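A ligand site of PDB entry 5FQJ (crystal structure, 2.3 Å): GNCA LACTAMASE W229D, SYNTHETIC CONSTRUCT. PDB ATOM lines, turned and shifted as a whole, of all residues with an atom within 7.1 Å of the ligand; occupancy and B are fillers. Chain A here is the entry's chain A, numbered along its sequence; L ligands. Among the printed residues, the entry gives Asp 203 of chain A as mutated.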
ATOM      1  N   VAL A  23      17.811 -23.371 -17.216  1.00  0.00           N
ATOM      2  CA  VAL A  23      16.793 -22.413 -17.628  1.00  0.00           C
ATOM      3  C   VAL A  23      16.250 -22.889 -18.955  1.00  0.00           C
ATOM      4  O   VAL A  23      16.996 -22.935 -19.947  1.00  0.00           O
ATOM      5  CB  VAL A  23      17.359 -20.982 -17.757  1.00  0.00           C
ATOM      6  CG1 VAL A  23      16.226 -20.001 -17.960  1.00  0.00           C
ATOM      7  CG2 VAL A  23      18.186 -20.603 -16.520  1.00  0.00           C
ATOM      8  N   LEU A  24      14.971 -23.245 -18.997  1.00  0.00           N
ATOM      9  CA  LEU A  24      14.337 -23.784 -20.186  1.00  0.00           C
ATOM     10  C   LEU A  24      13.272 -22.783 -20.644  1.00  0.00           C
ATOM     11  O   LEU A  24      12.215 -22.666 -20.019  1.00  0.00           O
ATOM     12  CB  LEU A  24      13.744 -25.167 -19.899  1.00  0.00           C
ATOM     13  CG  LEU A  24      13.654 -26.126 -21.065  1.00  0.00           C
ATOM     14  CD1 LEU A  24      13.055 -27.426 -20.600  1.00  0.00           C
ATOM     15  CD2 LEU A  24      12.841 -25.515 -22.207  1.00  0.00           C
ATOM     16  N   LEU A 195      14.209 -18.467  -5.254  1.00  0.00           N
ATOM     17  CA  LEU A 195      14.003 -17.898  -6.578  1.00  0.00           C
ATOM     18  C   LEU A 195      13.002 -16.751  -6.525  1.00  0.00           C
ATOM     19  O   LEU A 195      13.266 -15.668  -7.030  1.00  0.00           O
ATOM     20  CB  LEU A 195      13.540 -18.982  -7.557  1.00  0.00           C
ATOM     21  CG  LEU A 195      14.662 -19.855  -8.106  1.00  0.00           C
ATOM     22  CD1 LEU A 195      14.102 -20.998  -8.910  1.00  0.00           C
ATOM     23  CD2 LEU A 195      15.640 -19.046  -8.963  1.00  0.00           C
ATOM     24  N   LEU A 199      13.078 -12.557  -8.338  1.00  0.00           N
ATOM     25  CA  LEU A 199      12.319 -12.369  -9.562  1.00  0.00           C
ATOM     26  C   LEU A 199      11.463 -11.119  -9.503  1.00  0.00           C
ATOM     27  O   LEU A 199      11.241 -10.539  -8.434  1.00  0.00           O
ATOM     28  CB  LEU A 199      11.421 -13.580  -9.815  1.00  0.00           C
ATOM     29  CG  LEU A 199      12.129 -14.882 -10.155  1.00  0.00           C
ATOM     30  CD1 LEU A 199      11.113 -16.012 -10.223  1.00  0.00           C
ATOM     31  CD2 LEU A 199      12.884 -14.764 -11.456  1.00  0.00           C
ATOM     32  N   PRO A 200      10.968 -10.659 -10.656  1.00  0.00           N
ATOM     33  CA  PRO A 200       9.984  -9.585 -10.659  1.00  0.00           C
ATOM     34  C   PRO A 200       8.674 -10.025 -10.003  1.00  0.00           C
ATOM     35  O   PRO A 200       8.198 -11.143 -10.207  1.00  0.00           O
ATOM     36  CB  PRO A 200       9.795  -9.271 -12.146  1.00  0.00           C
ATOM     37  CG  PRO A 200      11.072  -9.746 -12.789  1.00  0.00           C
ATOM     38  CD  PRO A 200      11.490 -10.948 -12.009  1.00  0.00           C
ATOM     39  N   ASP A 202       5.658  -9.001 -10.579  1.00  0.00           N
ATOM     40  CA  ASP A 202       4.581  -9.203 -11.539  1.00  0.00           C
ATOM     41  C   ASP A 202       4.551 -10.616 -12.105  1.00  0.00           C
ATOM     42  O   ASP A 202       3.622 -10.940 -12.845  1.00  0.00           O
ATOM     43  CB  ASP A 202       4.692  -8.205 -12.680  1.00  0.00           C
ATOM     44  CG  ASP A 202       4.279  -6.799 -12.277  1.00  0.00           C
ATOM     45  OD1 ASP A 202       4.053  -6.574 -11.067  1.00  0.00           O
ATOM     46  OD2 ASP A 202       4.206  -5.916 -13.163  1.00  0.00           O
ATOM     47  N   ASP A 203       5.541 -11.447 -11.791  1.00  0.00           N
ATOM     48  CA  ASP A 203       5.580 -12.800 -12.320  1.00  0.00           C
ATOM     49  C   ASP A 203       4.677 -13.726 -11.523  1.00  0.00           C
ATOM     50  O   ASP A 203       4.550 -13.600 -10.305  1.00  0.00           O
ATOM     51  CB  ASP A 203       7.004 -13.352 -12.271  1.00  0.00           C
ATOM     52  CG  ASP A 203       7.924 -12.686 -13.256  1.00  0.00           C
ATOM     53  OD1 ASP A 203       7.434 -11.911 -14.104  1.00  0.00           O
ATOM     54  OD2 ASP A 203       9.140 -12.957 -13.185  1.00  0.00           O
ATOM     55  N   ILE A 223       7.963 -20.284 -14.277  1.00  0.00           N
ATOM     56  CA  ILE A 223       7.726 -18.850 -14.127  1.00  0.00           C
ATOM     57  C   ILE A 223       6.940 -18.366 -15.342  1.00  0.00           C
ATOM     58  O   ILE A 223       7.302 -18.679 -16.480  1.00  0.00           O
ATOM     59  CB  ILE A 223       9.069 -18.098 -13.993  1.00  0.00           C
ATOM     60  CG1 ILE A 223       9.888 -18.721 -12.866  1.00  0.00           C
ATOM     61  CG2 ILE A 223       8.827 -16.614 -13.762  1.00  0.00           C
ATOM     62  CD1 ILE A 223      11.312 -18.247 -12.816  1.00  0.00           C
ATOM     63  N   TRP A 224       5.859 -17.627 -15.094  1.00  0.00           N
ATOM     64  CA  TRP A 224       5.048 -17.051 -16.162  1.00  0.00           C
ATOM     65  C   TRP A 224       5.223 -15.544 -16.133  1.00  0.00           C
ATOM     66  O   TRP A 224       4.544 -14.839 -15.381  1.00  0.00           O
ATOM     67  CB  TRP A 224       3.565 -17.412 -16.014  1.00  0.00           C
ATOM     68  CG  TRP A 224       3.223 -18.829 -16.243  1.00  0.00           C
ATOM     69  CD1 TRP A 224       2.738 -19.373 -17.398  1.00  0.00           C
ATOM     70  CD2 TRP A 224       3.301 -19.902 -15.300  1.00  0.00           C
ATOM     71  NE1 TRP A 224       2.524 -20.722 -17.230  1.00  0.00           N
ATOM     72  CE2 TRP A 224       2.861 -21.070 -15.953  1.00  0.00           C
ATOM     73  CE3 TRP A 224       3.702 -19.986 -13.971  1.00  0.00           C
ATOM     74  CZ2 TRP A 224       2.806 -22.305 -15.313  1.00  0.00           C
ATOM     75  CZ3 TRP A 224       3.660 -21.227 -13.334  1.00  0.00           C
ATOM     76  CH2 TRP A 224       3.220 -22.363 -14.015  1.00  0.00           C
ATOM     77  N   PRO A 225       6.152 -14.994 -16.927  1.00  0.00           N
ATOM     78  CA  PRO A 225       6.263 -13.541 -16.995  1.00  0.00           C
ATOM     79  C   PRO A 225       5.111 -12.940 -17.765  1.00  0.00           C
ATOM     80  O   PRO A 225       4.564 -13.580 -18.695  1.00  0.00           O
ATOM     81  CB  PRO A 225       7.604 -13.319 -17.726  1.00  0.00           C
ATOM     82  CG  PRO A 225       8.316 -14.621 -17.653  1.00  0.00           C
ATOM     83  CD  PRO A 225       7.249 -15.662 -17.640  1.00  0.00           C
ATOM     84  N   PRO A 226       4.697 -11.720 -17.439  1.00  0.00           N
ATOM     85  CA  PRO A 226       3.544 -11.112 -18.132  1.00  0.00           C
ATOM     86  C   PRO A 226       3.749 -11.056 -19.642  1.00  0.00           C
ATOM     87  O   PRO A 226       4.766 -10.575 -20.134  1.00  0.00           O
ATOM     88  CB  PRO A 226       3.465  -9.719 -17.515  1.00  0.00           C
ATOM     89  CG  PRO A 226       4.213  -9.824 -16.200  1.00  0.00           C
ATOM     90  CD  PRO A 226       5.298 -10.803 -16.460  1.00  0.00           C
ATOM     91  N   ARG A 228       4.427 -13.250 -21.789  1.00  0.00           N
ATOM     92  CA  ARG A 228       5.590 -13.977 -22.248  1.00  0.00           C
ATOM     93  C   ARG A 228       5.364 -15.459 -22.039  1.00  0.00           C
ATOM     94  O   ARG A 228       4.651 -15.862 -21.103  1.00  0.00           O
ATOM     95  CB  ARG A 228       6.842 -13.528 -21.507  1.00  0.00           C
ATOM     96  CG  ARG A 228       8.096 -14.050 -22.119  1.00  0.00           C
ATOM     97  CD  ARG A 228       9.255 -14.003 -21.181  1.00  0.00           C
ATOM     98  NE  ARG A 228      10.466 -14.230 -21.946  1.00  0.00           N
ATOM     99  CZ  ARG A 228      10.814 -15.402 -22.473  1.00  0.00           C
ATOM    100  NH1 ARG A 228      10.032 -16.476 -22.309  1.00  0.00           N
ATOM    101  NH2 ARG A 228      11.931 -15.494 -23.162  1.00  0.00           N
ATOM    102  N   ILE A 231       8.921 -19.960 -18.415  1.00  0.00           N
ATOM    103  CA  ILE A 231      10.325 -20.326 -18.314  1.00  0.00           C
ATOM    104  C   ILE A 231      10.479 -21.271 -17.136  1.00  0.00           C
ATOM    105  O   ILE A 231       9.918 -21.025 -16.061  1.00  0.00           O
ATOM    106  CB  ILE A 231      11.209 -19.069 -18.108  1.00  0.00           C
ATOM    107  CG1 ILE A 231      11.049 -18.090 -19.277  1.00  0.00           C
ATOM    108  CG2 ILE A 231      12.663 -19.474 -17.920  1.00  0.00           C
ATOM    109  CD1 ILE A 231      11.634 -16.707 -19.000  1.00  0.00           C
ATOM    110  N   VAL A 232      11.270 -22.323 -17.315  1.00  0.00           N
ATOM    111  CA  VAL A 232      11.536 -23.291 -16.263  1.00  0.00           C
ATOM    112  C   VAL A 232      12.947 -23.051 -15.742  1.00  0.00           C
ATOM    113  O   VAL A 232      13.919 -23.092 -16.503  1.00  0.00           O
ATOM    114  CB  VAL A 232      11.381 -24.743 -16.740  1.00  0.00           C
ATOM    115  CG1 VAL A 232      11.550 -25.691 -15.595  1.00  0.00           C
ATOM    116  CG2 VAL A 232      10.022 -24.955 -17.359  1.00  0.00           C
ATOM    117  N   VAL A 233      13.053 -22.815 -14.441  1.00  0.00           N
ATOM    118  CA  VAL A 233      14.339 -22.626 -13.779  1.00  0.00           C
ATOM    119  C   VAL A 233      14.501 -23.689 -12.706  1.00  0.00           C
ATOM    120  O   VAL A 233      13.645 -23.807 -11.820  1.00  0.00           O
ATOM    121  CB  VAL A 233      14.455 -21.225 -13.161  1.00  0.00           C
ATOM    122  CG1 VAL A 233      15.829 -21.052 -12.572  1.00  0.00           C
ATOM    123  CG2 VAL A 233      14.151 -20.154 -14.210  1.00  0.00           C
ATOM    124  N   GLY A 255      18.307 -16.330  -9.393  1.00  0.00           N
ATOM    125  CA  GLY A 255      17.097 -15.778  -9.977  1.00  0.00           C
ATOM    126  C   GLY A 255      17.327 -14.411 -10.578  1.00  0.00           C
ATOM    127  O   GLY A 255      16.957 -14.149 -11.724  1.00  0.00           O
ATOM    128  N   VAL A 258      19.383 -14.646 -13.654  1.00  0.00           N
ATOM    129  CA  VAL A 258      18.677 -15.223 -14.801  1.00  0.00           C
ATOM    130  C   VAL A 258      17.820 -14.171 -15.488  1.00  0.00           C
ATOM    131  O   VAL A 258      17.750 -14.112 -16.723  1.00  0.00           O
ATOM    132  CB  VAL A 258      17.854 -16.446 -14.355  1.00  0.00           C
ATOM    133  CG1 VAL A 258      16.869 -16.857 -15.455  1.00  0.00           C
ATOM    134  CG2 VAL A 258      18.777 -17.627 -14.004  1.00  0.00           C
ATOM    135  N   VAL A 259      17.186 -13.301 -14.704  1.00  0.00           N
ATOM    136  CA  VAL A 259      16.350 -12.251 -15.265  1.00  0.00           C
ATOM    137  C   VAL A 259      17.211 -11.247 -16.024  1.00  0.00           C
ATOM    138  O   VAL A 259      16.902 -10.873 -17.169  1.00  0.00           O
ATOM    139  CB  VAL A 259      15.537 -11.573 -14.155  1.00  0.00           C
ATOM    140  CG1 VAL A 259      14.694 -10.439 -14.710  1.00  0.00           C
ATOM    141  CG2 VAL A 259      14.658 -12.603 -13.454  1.00  0.00           C
ATOM    142  N   GLU A 260      18.296 -10.786 -15.402  1.00  0.00           N
ATOM    143  CA  GLU A 260      19.204  -9.851 -16.064  1.00  0.00           C
ATOM    144  C   GLU A 260      19.671 -10.393 -17.417  1.00  0.00           C
ATOM    145  O   GLU A 260      19.745  -9.639 -18.402  1.00  0.00           O
ATOM    146  CB  GLU A 260      20.408  -9.546 -15.176  1.00  0.00           C
ATOM    147  CG  GLU A 260      20.111  -8.540 -14.080  1.00  0.00           C
ATOM    148  CD  GLU A 260      21.211  -7.519 -13.918  1.00  0.00           C
ATOM    149  OE1 GLU A 260      22.362  -7.915 -13.612  1.00  0.00           O
ATOM    150  OE2 GLU A 260      20.928  -6.314 -14.111  1.00  0.00           O
ATOM    151  N   ALA A 261      19.997 -11.678 -17.487  1.00  0.00           N
ATOM    152  CA  ALA A 261      20.504 -12.240 -18.732  1.00  0.00           C
ATOM    153  C   ALA A 261      19.405 -12.328 -19.803  1.00  0.00           C
ATOM    154  O   ALA A 261      19.710 -12.292 -20.993  1.00  0.00           O
ATOM    155  CB  ALA A 261      21.131 -13.607 -18.486  1.00  0.00           C
ATOM    156  N   PHE A 262      18.139 -12.458 -19.401  1.00  0.00           N
ATOM    157  CA  PHE A 262      17.066 -12.466 -20.390  1.00  0.00           C
ATOM    158  C   PHE A 262      16.823 -11.082 -20.963  1.00  0.00           C
ATOM    159  O   PHE A 262      16.372 -10.962 -22.107  1.00  0.00           O
ATOM    160  CB  PHE A 262      15.769 -12.994 -19.778  1.00  0.00           C
ATOM    161  CG  PHE A 262      15.522 -14.443 -20.047  1.00  0.00           C
ATOM    162  CD1 PHE A 262      16.165 -15.417 -19.304  1.00  0.00           C
ATOM    163  CD2 PHE A 262      14.651 -14.840 -21.035  1.00  0.00           C
ATOM    164  CE1 PHE A 262      15.926 -16.761 -19.550  1.00  0.00           C
ATOM    165  CE2 PHE A 262      14.414 -16.176 -21.286  1.00  0.00           C
ATOM    166  CZ  PHE A 262      15.050 -17.138 -20.529  1.00  0.00           C
ATOM    167  N   HIS A 263      17.119 -10.043 -20.194  1.00  0.00           N
ATOM    168  CA  HIS A 263      16.817  -8.678 -20.609  1.00  0.00           C
ATOM    169  C   HIS A 263      17.998  -7.958 -21.248  1.00  0.00           C
ATOM    170  O   HIS A 263      17.785  -7.076 -22.087  1.00  0.00           O
ATOM    171  CB  HIS A 263      16.349  -7.860 -19.401  1.00  0.00           C
ATOM    172  CG  HIS A 263      14.966  -8.205 -18.936  1.00  0.00           C
ATOM    173  ND1 HIS A 263      13.871  -7.415 -19.208  1.00  0.00           N
ATOM    174  CD2 HIS A 263      14.507  -9.251 -18.217  1.00  0.00           C
ATOM    175  CE1 HIS A 263      12.794  -7.961 -18.674  1.00  0.00           C
ATOM    176  NE2 HIS A 263      13.143  -9.082 -18.069  1.00  0.00           N
HETATM  177  O1  LIG L   1      13.067 -16.628 -14.570  1.00  0.00           O
HETATM  178  N1  LIG L   1      13.320 -16.229 -15.653  1.00  0.00           N
HETATM  179  O2  LIG L   1      14.037 -16.880 -16.421  1.00  0.00           O
HETATM  180  C1  LIG L   1      12.805 -14.908 -16.173  1.00  0.00           C
HETATM  181  C2  LIG L   1      13.397 -14.306 -17.301  1.00  0.00           C
HETATM  182  C3  LIG L   1      12.913 -13.092 -17.783  1.00  0.00           C
HETATM  183  C4  LIG L   1      11.824 -12.475 -17.134  1.00  0.00           C
HETATM  184  N2  LIG L   1      11.089 -11.255 -17.344  1.00  0.00           N
HETATM  185  C5  LIG L   1      11.253 -13.104 -16.001  1.00  0.00           C
HETATM  186  C6  LIG L   1      11.740 -14.324 -15.526  1.00  0.00           C
HETATM  187  N3  LIG L   1      10.220 -12.254 -15.602  1.00  0.00           N
HETATM  188  N4  LIG L   1      10.184 -11.179 -16.441  1.00  0.00           N
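N3 of the ligand sits at hydrogen-bond distance from OD2 of Asp 203.
A ring nitrogen (NE2) of His 263 sits at hydrogen-bond distance from a nitrogen (N2) of the ligand (3.1 Å).
N of Ile 223 sits at hydrogen-bond distance from O of Ile 231, at 2.7 Å.
Residues that only touch the ligand: Ile 223, Val 258, Ile 231, Phe 262, Pro 225, Leu 199, Val 233, Pro 200 and Val 259.
Hydrophobic or aromatic side chains that line the ligand: Leu 199, Pro 200, Ile 223, Pro 225, Ile 231, Val 233, Val 258, Val 259, Phe 262 and His 263.
The nearest printed residue that does not touch the ligand is Val 23 (4.1 Å).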
